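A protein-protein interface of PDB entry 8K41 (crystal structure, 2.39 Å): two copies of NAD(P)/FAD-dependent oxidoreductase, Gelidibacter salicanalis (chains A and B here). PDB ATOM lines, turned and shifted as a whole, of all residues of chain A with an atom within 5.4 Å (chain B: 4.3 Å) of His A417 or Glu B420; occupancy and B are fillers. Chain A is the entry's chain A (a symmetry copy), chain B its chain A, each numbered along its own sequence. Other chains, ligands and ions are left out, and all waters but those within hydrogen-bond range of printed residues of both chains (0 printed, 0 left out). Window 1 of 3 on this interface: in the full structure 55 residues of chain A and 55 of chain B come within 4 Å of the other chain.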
ATOM      1  N   THR A 356     -18.421  14.497  14.470  1.00  0.00           N
ATOM      2  CA  THR A 356     -16.969  14.809  14.484  1.00  0.00           C
ATOM      3  C   THR A 356     -16.248  13.749  13.669  1.00  0.00           C
ATOM      4  O   THR A 356     -16.745  12.615  13.661  1.00  0.00           O
ATOM      5  CB  THR A 356     -16.378  14.797  15.896  1.00  0.00           C
ATOM      6  OG1 THR A 356     -16.647  13.503  16.449  1.00  0.00           O
ATOM      7  CG2 THR A 356     -16.957  15.892  16.763  1.00  0.00           C
ATOM      8  N   LEU A 390     -27.825   6.352  19.634  1.00  0.00           N
ATOM      9  CA  LEU A 390     -27.737   7.833  19.474  1.00  0.00           C
ATOM     10  C   LEU A 390     -28.350   8.276  18.125  1.00  0.00           C
ATOM     11  O   LEU A 390     -28.498   9.498  17.925  1.00  0.00           O
ATOM     12  CB  LEU A 390     -26.267   8.267  19.596  1.00  0.00           C
ATOM     13  CG  LEU A 390     -25.544   7.886  20.887  1.00  0.00           C
ATOM     14  CD1 LEU A 390     -24.072   8.276  20.829  1.00  0.00           C
ATOM     15  CD2 LEU A 390     -26.199   8.530  22.093  1.00  0.00           C
ATOM     16  N   GLY A 415     -17.836   9.629  13.734  1.00  0.00           N
ATOM     17  CA  GLY A 415     -18.958   9.137  14.563  1.00  0.00           C
ATOM     18  C   GLY A 415     -19.013   9.859  15.899  1.00  0.00           C
ATOM     19  O   GLY A 415     -18.422  10.938  16.031  1.00  0.00           O
ATOM     20  N   PRO A 416     -19.736   9.290  16.892  1.00  0.00           N
ATOM     21  CA  PRO A 416     -19.831   9.860  18.233  1.00  0.00           C
ATOM     22  C   PRO A 416     -18.509   9.834  19.008  1.00  0.00           C
ATOM     23  O   PRO A 416     -17.778   8.821  18.887  1.00  0.00           O
ATOM     24  CB  PRO A 416     -20.812   8.958  18.994  1.00  0.00           C
ATOM     25  CG  PRO A 416     -21.462   8.078  17.948  1.00  0.00           C
ATOM     26  CD  PRO A 416     -20.550   8.074  16.745  1.00  0.00           C
ATOM     27  N   HIS A 417     -18.264  10.918  19.774  1.00  0.00           N
ATOM     28  CA  HIS A 417     -17.155  11.113  20.744  1.00  0.00           C
ATOM     29  C   HIS A 417     -15.779  10.837  20.099  1.00  0.00           C
ATOM     30  O   HIS A 417     -14.824  10.671  20.833  1.00  0.00           O
ATOM     31  CB  HIS A 417     -17.419  10.295  22.030  1.00  0.00           C
ATOM     32  CG  HIS A 417     -18.737  10.582  22.673  1.00  0.00           C
ATOM     33  ND1 HIS A 417     -19.332  11.835  22.622  1.00  0.00           N
ATOM     34  CD2 HIS A 417     -19.592   9.790  23.359  1.00  0.00           C
ATOM     35  CE1 HIS A 417     -20.495  11.799  23.245  1.00  0.00           C
ATOM     36  NE2 HIS A 417     -20.681  10.553  23.704  1.00  0.00           N
ATOM     37  N   THR A 418     -15.641  10.903  18.778  1.00  0.00           N
ATOM     38  CA  THR A 418     -14.372  10.569  18.081  1.00  0.00           C
ATOM     39  C   THR A 418     -13.262  11.532  18.513  1.00  0.00           C
ATOM     40  O   THR A 418     -12.128  11.067  18.698  1.00  0.00           O
ATOM     41  CB  THR A 418     -14.566  10.518  16.564  1.00  0.00           C
ATOM     42  OG1 THR A 418     -14.773  11.830  16.027  1.00  0.00           O
ATOM     43  CG2 THR A 418     -15.691   9.579  16.184  1.00  0.00           C
ATOM     44  N   GLU A 419     -13.596  12.807  18.726  1.00  0.00           N
ATOM     45  CA  GLU A 419     -12.639  13.837  19.202  1.00  0.00           C
ATOM     46  C   GLU A 419     -12.016  13.371  20.532  1.00  0.00           C
ATOM     47  O   GLU A 419     -10.834  13.686  20.774  1.00  0.00           O
ATOM     48  CB  GLU A 419     -13.308  15.210  19.268  1.00  0.00           C
ATOM     49  CG  GLU A 419     -14.146  15.445  20.507  1.00  0.00           C
ATOM     50  CD  GLU A 419     -15.601  14.994  20.490  1.00  0.00           C
ATOM     51  OE1 GLU A 419     -16.333  15.343  21.467  1.00  0.00           O
ATOM     52  OE2 GLU A 419     -16.015  14.322  19.519  1.00  0.00           O
ATOM     53  N   GLU A 420     -12.756  12.627  21.349  1.00  0.00           N
ATOM     54  CA  GLU A 420     -12.244  12.021  22.606  1.00  0.00           C
ATOM     55  C   GLU A 420     -11.471  10.749  22.279  1.00  0.00           C
ATOM     56  O   GLU A 420     -10.269  10.693  22.577  1.00  0.00           O
ATOM     57  CB  GLU A 420     -13.401  11.737  23.557  1.00  0.00           C
ATOM     58  CG  GLU A 420     -14.153  13.000  23.952  1.00  0.00           C
ATOM     59  CD  GLU A 420     -13.376  13.934  24.861  1.00  0.00           C
ATOM     60  OE1 GLU A 420     -13.721  15.133  24.895  1.00  0.00           O
ATOM     61  OE2 GLU A 420     -12.409  13.460  25.523  1.00  0.00           O
ATOM     62  N   THR A 421     -12.142   9.793  21.634  1.00  0.00           N
ATOM     63  CA  THR A 421     -11.640   8.426  21.352  1.00  0.00           C
ATOM     64  C   THR A 421     -10.269   8.487  20.649  1.00  0.00           C
ATOM     65  O   THR A 421      -9.386   7.629  20.928  1.00  0.00           O
ATOM     66  CB  THR A 421     -12.721   7.669  20.574  1.00  0.00           C
ATOM     67  OG1 THR A 421     -13.989   8.030  21.117  1.00  0.00           O
ATOM     68  CG2 THR A 421     -12.564   6.169  20.670  1.00  0.00           C
ATOM     69  N   ILE A 422     -10.056   9.484  19.797  1.00  0.00           N
ATOM     70  CA  ILE A 422      -8.821   9.547  18.978  1.00  0.00           C
ATOM     71  C   ILE A 422      -7.600   9.597  19.888  1.00  0.00           C
ATOM     72  O   ILE A 422      -6.541   9.167  19.433  1.00  0.00           O
ATOM     73  CB  ILE A 422      -8.838  10.726  17.987  1.00  0.00           C
ATOM     74  CG1 ILE A 422      -7.753  10.548  16.921  1.00  0.00           C
ATOM     75  CG2 ILE A 422      -8.737  12.060  18.702  1.00  0.00           C
ATOM     76  CD1 ILE A 422      -8.088   9.482  15.879  1.00  0.00           C
ATOM     77  N   LEU A 424      -6.954   7.903  22.597  1.00  0.00           N
ATOM     78  CA  LEU A 424      -6.594   6.519  23.013  1.00  0.00           C
ATOM     79  C   LEU A 424      -5.673   5.932  21.956  1.00  0.00           C
ATOM     80  O   LEU A 424      -4.788   5.112  22.293  1.00  0.00           O
ATOM     81  CB  LEU A 424      -7.864   5.675  23.154  1.00  0.00           C
ATOM     82  CG  LEU A 424      -8.721   6.022  24.367  1.00  0.00           C
ATOM     83  CD1 LEU A 424     -10.198   5.948  24.043  1.00  0.00           C
ATOM     84  CD2 LEU A 424      -8.349   5.128  25.543  1.00  0.00           C
ATOM     85  N   SER A 444     -14.484   0.627  30.371  1.00  0.00           N
ATOM     86  CA  SER A 444     -15.860   1.036  30.729  1.00  0.00           C
ATOM     87  C   SER A 444     -16.776   0.661  29.570  1.00  0.00           C
ATOM     88  O   SER A 444     -16.389   0.884  28.411  1.00  0.00           O
ATOM     89  CB  SER A 444     -15.921   2.494  30.981  1.00  0.00           C
ATOM     90  OG  SER A 444     -15.364   3.215  29.882  1.00  0.00           O
ATOM     91  N   THR A 447     -19.663   2.459  26.380  1.00  0.00           N
ATOM     92  CA  THR A 447     -18.921   3.631  25.858  1.00  0.00           C
ATOM     93  C   THR A 447     -18.441   3.421  24.414  1.00  0.00           C
ATOM     94  O   THR A 447     -18.276   2.262  23.986  1.00  0.00           O
ATOM     95  CB  THR A 447     -17.657   3.895  26.669  1.00  0.00           C
ATOM     96  OG1 THR A 447     -16.751   2.839  26.353  1.00  0.00           O
ATOM     97  CG2 THR A 447     -17.935   3.996  28.147  1.00  0.00           C
ATOM     98  N   LEU A 448     -18.197   4.526  23.712  1.00  0.00           N
ATOM     99  CA  LEU A 448     -17.545   4.576  22.377  1.00  0.00           C
ATOM    100  C   LEU A 448     -16.120   4.003  22.475  1.00  0.00           C
ATOM    101  O   LEU A 448     -15.720   3.260  21.601  1.00  0.00           O
ATOM    102  CB  LEU A 448     -17.507   6.034  21.918  1.00  0.00           C
ATOM    103  CG  LEU A 448     -18.737   6.517  21.157  1.00  0.00           C
ATOM    104  CD1 LEU A 448     -18.777   5.869  19.782  1.00  0.00           C
ATOM    105  CD2 LEU A 448     -20.025   6.238  21.928  1.00  0.00           C
ATOM    106  N   ALA A 449     -15.393   4.296  23.540  1.00  0.00           N
ATOM    107  CA  ALA A 449     -14.039   3.750  23.788  1.00  0.00           C
ATOM    108  C   ALA A 449     -14.049   2.225  23.676  1.00  0.00           C
ATOM    109  O   ALA A 449     -13.003   1.654  23.269  1.00  0.00           O
ATOM    110  CB  ALA A 449     -13.551   4.206  25.136  1.00  0.00           C
ATOM    111  N   HIS B 417     -17.962  13.598  29.925  1.00  0.00           N
ATOM    112  CA  HIS B 417     -17.303  12.526  29.134  1.00  0.00           C
ATOM    113  C   HIS B 417     -16.374  11.659  30.012  1.00  0.00           C
ATOM    114  O   HIS B 417     -15.559  10.947  29.457  1.00  0.00           O
ATOM    115  CB  HIS B 417     -16.606  13.129  27.892  1.00  0.00           C
ATOM    116  CG  HIS B 417     -17.510  13.944  27.024  1.00  0.00           C
ATOM    117  ND1 HIS B 417     -18.859  13.656  26.878  1.00  0.00           N
ATOM    118  CD2 HIS B 417     -17.280  15.047  26.274  1.00  0.00           C
ATOM    119  CE1 HIS B 417     -19.419  14.546  26.080  1.00  0.00           C
ATOM    120  NE2 HIS B 417     -18.471  15.415  25.699  1.00  0.00           N
ATOM    121  N   THR B 418     -16.558  11.616  31.328  1.00  0.00           N
ATOM    122  CA  THR B 418     -15.655  10.873  32.245  1.00  0.00           C
ATOM    123  C   THR B 418     -15.689   9.376  31.922  1.00  0.00           C
ATOM    124  O   THR B 418     -14.621   8.748  31.960  1.00  0.00           O
ATOM    125  CB  THR B 418     -15.975  11.177  33.711  1.00  0.00           C
ATOM    126  OG1 THR B 418     -17.219  10.585  34.100  1.00  0.00           O
ATOM    127  CG2 THR B 418     -15.959  12.667  33.979  1.00  0.00           C
ATOM    128  N   GLU B 419     -16.859   8.847  31.556  1.00  0.00           N
ATOM    129  CA  GLU B 419     -17.028   7.426  31.160  1.00  0.00           C
ATOM    130  C   GLU B 419     -16.078   7.112  29.990  1.00  0.00           C
ATOM    131  O   GLU B 419     -15.588   5.967  29.917  1.00  0.00           O
ATOM    132  CB  GLU B 419     -18.500   7.114  30.878  1.00  0.00           C
ATOM    133  CG  GLU B 419     -18.981   7.534  29.506  1.00  0.00           C
ATOM    134  CD  GLU B 419     -19.489   8.958  29.325  1.00  0.00           C
ATOM    135  OE1 GLU B 419     -20.040   9.246  28.217  1.00  0.00           O
ATOM    136  OE2 GLU B 419     -19.359   9.772  30.265  1.00  0.00           O
ATOM    137  N   GLU B 420     -15.797   8.083  29.127  1.00  0.00           N
ATOM    138  CA  GLU B 420     -14.813   7.947  28.021  1.00  0.00           C
ATOM    139  C   GLU B 420     -13.403   8.136  28.569  1.00  0.00           C
ATOM    140  O   GLU B 420     -12.600   7.197  28.473  1.00  0.00           O
ATOM    141  CB  GLU B 420     -15.121   8.958  26.921  1.00  0.00           C
ATOM    142  CG  GLU B 420     -16.499   8.752  26.310  1.00  0.00           C
ATOM    143  CD  GLU B 420     -16.630   7.497  25.468  1.00  0.00           C
ATOM    144  OE1 GLU B 420     -17.776   7.038  25.282  1.00  0.00           O
ATOM    145  OE2 GLU B 420     -15.576   6.969  25.010  1.00  0.00           O
ATOM    146  N   THR B 421     -13.150   9.299  29.172  1.00  0.00           N
ATOM    147  CA  THR B 421     -11.819   9.757  29.639  1.00  0.00           C
ATOM    148  C   THR B 421     -11.168   8.694  30.547  1.00  0.00           C
ATOM    149  O   THR B 421      -9.924   8.496  30.483  1.00  0.00           O
ATOM    150  CB  THR B 421     -11.986  11.133  30.291  1.00  0.00           C
ATOM    151  OG1 THR B 421     -12.934  11.871  29.523  1.00  0.00           O
ATOM    152  CG2 THR B 421     -10.693  11.914  30.342  1.00  0.00           C
ATOM    153  N   ILE B 422     -11.966   7.987  31.339  1.00  0.00           N
ATOM    154  CA  ILE B 422     -11.417   7.038  32.339  1.00  0.00           C
ATOM    155  C   ILE B 422     -10.587   5.972  31.637  1.00  0.00           C
ATOM    156  O   ILE B 422      -9.695   5.434  32.289  1.00  0.00           O
ATOM    157  CB  ILE B 422     -12.518   6.414  33.217  1.00  0.00           C
ATOM    158  CG1 ILE B 422     -11.907   5.751  34.454  1.00  0.00           C
ATOM    159  CG2 ILE B 422     -13.396   5.466  32.423  1.00  0.00           C
ATOM    160  CD1 ILE B 422     -11.431   6.747  35.511  1.00  0.00           C
ATOM    161  N   ASN B 423     -10.894   5.653  30.370  1.00  0.00           N
ATOM    162  CA  ASN B 423     -10.184   4.570  29.632  1.00  0.00           C
ATOM    163  C   ASN B 423      -8.718   4.975  29.384  1.00  0.00           C
ATOM    164  O   ASN B 423      -7.864   4.073  29.420  1.00  0.00           O
ATOM    165  CB  ASN B 423     -10.958   4.140  28.389  1.00  0.00           C
ATOM    166  CG  ASN B 423     -12.333   3.619  28.758  1.00  0.00           C
ATOM    167  OD1 ASN B 423     -12.447   2.542  29.355  1.00  0.00           O
ATOM    168  ND2 ASN B 423     -13.373   4.392  28.451  1.00  0.00           N
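The side-chain carboxylate (OE2) of Glu B420 lies within hydrogen-bond range of the backbone NH (N) of Ala A449 (3.1 Å).
The backbone NH (N) of Leu A448 is in hydrogen-bond range of the side-chain carboxylate (OE1) of Glu B420, at 3.0 Å.
The side-chain amide nitrogen (ND2) of Asn B423 sits at hydrogen-bond distance from the side-chain hydroxyl (OG) of Ser A444 (2.7 Å).
O of Glu B419 sits at hydrogen-bond distance from OG of Ser A444.
O of His A417 lies within hydrogen-bond range of OG1 of Thr A421 (2.8 Å).
The side-chain hydroxyl of Thr A447 lies close to the backbone NH of Ala A449 (3.4 Å).
The side-chain amide nitrogen of Asn B423 lies within hydrogen-bond range of the backbone carbonyl oxygen of Glu B419.
The backbone carbonyl oxygen of Glu B420 is in hydrogen-bond range of the side-chain amide nitrogen of Asn B423 (2.9 Å).
The side-chain hydroxyl (OG1) of Thr A447 lies within hydrogen-bond range of the backbone carbonyl oxygen (O) of Ser A444, 2.9 Å away.
The side-chain hydroxyl of Thr B421 sits at hydrogen-bond distance from the backbone carbonyl oxygen of His B417 (2.8 Å).
Among the printed residues, pairs that only touch across the chains: Ala A449 with Asn B423 (3.3 Å), Thr A447 with Glu B420 (3.4 Å), Thr A447 with Glu B419 (3.5 Å), His A417 with Glu B420 (3.8 Å), Glu A420 with His B417 (3.8 Å), Leu A424 with Asn B423 (3.9 Å) and Ser A444 with Ile B422 (3.9 Å).
Glu B420 touches just these residues of chain A: His A417, Thr A447, Leu A448 and Ala A449.
Printed residues of chain B within 4 Å of Thr A447: Glu B419 (3.5 Å) and Glu B420 (3.4 Å).
Of the printed residues of chain B, Leu A424 touches Asn B423 (3.9 Å).
Of the printed residues of chain A, Ile B422 touches Ser A444 (3.9 Å).
Of the printed residues of chain B, Glu A420 touches His B417.
Of the printed residues of chain B, Ala A449 touches Glu B420 (3.1 Å) and Asn B423 (3.3 Å).
Thr B421 touches none of the printed residues of chain A.
The nearest printed residue of chain B that does not touch Glu A420 is Thr B421 (4.3 Å).
Of the 15 printed residues of chain A, 7 touch a printed residue of chain B.
Hydrophobic or aromatic side chains of chain A within 4 Å of the printed part of chain B: His A417, Leu A424, Leu A448 and Ala A449.
Of the 7 printed residues of chain B, 5 touch a printed residue of chain A.
Hydrophobic or aromatic side chains of chain B within 4 Å of the printed part of chain A: His B417 and Ile B422.
His A417 touches Glu B420, and with the chains exchanged Glu A420 touches His B417.
Positions printed for both chains: 417, 418, 419, 420, 421 and 422.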
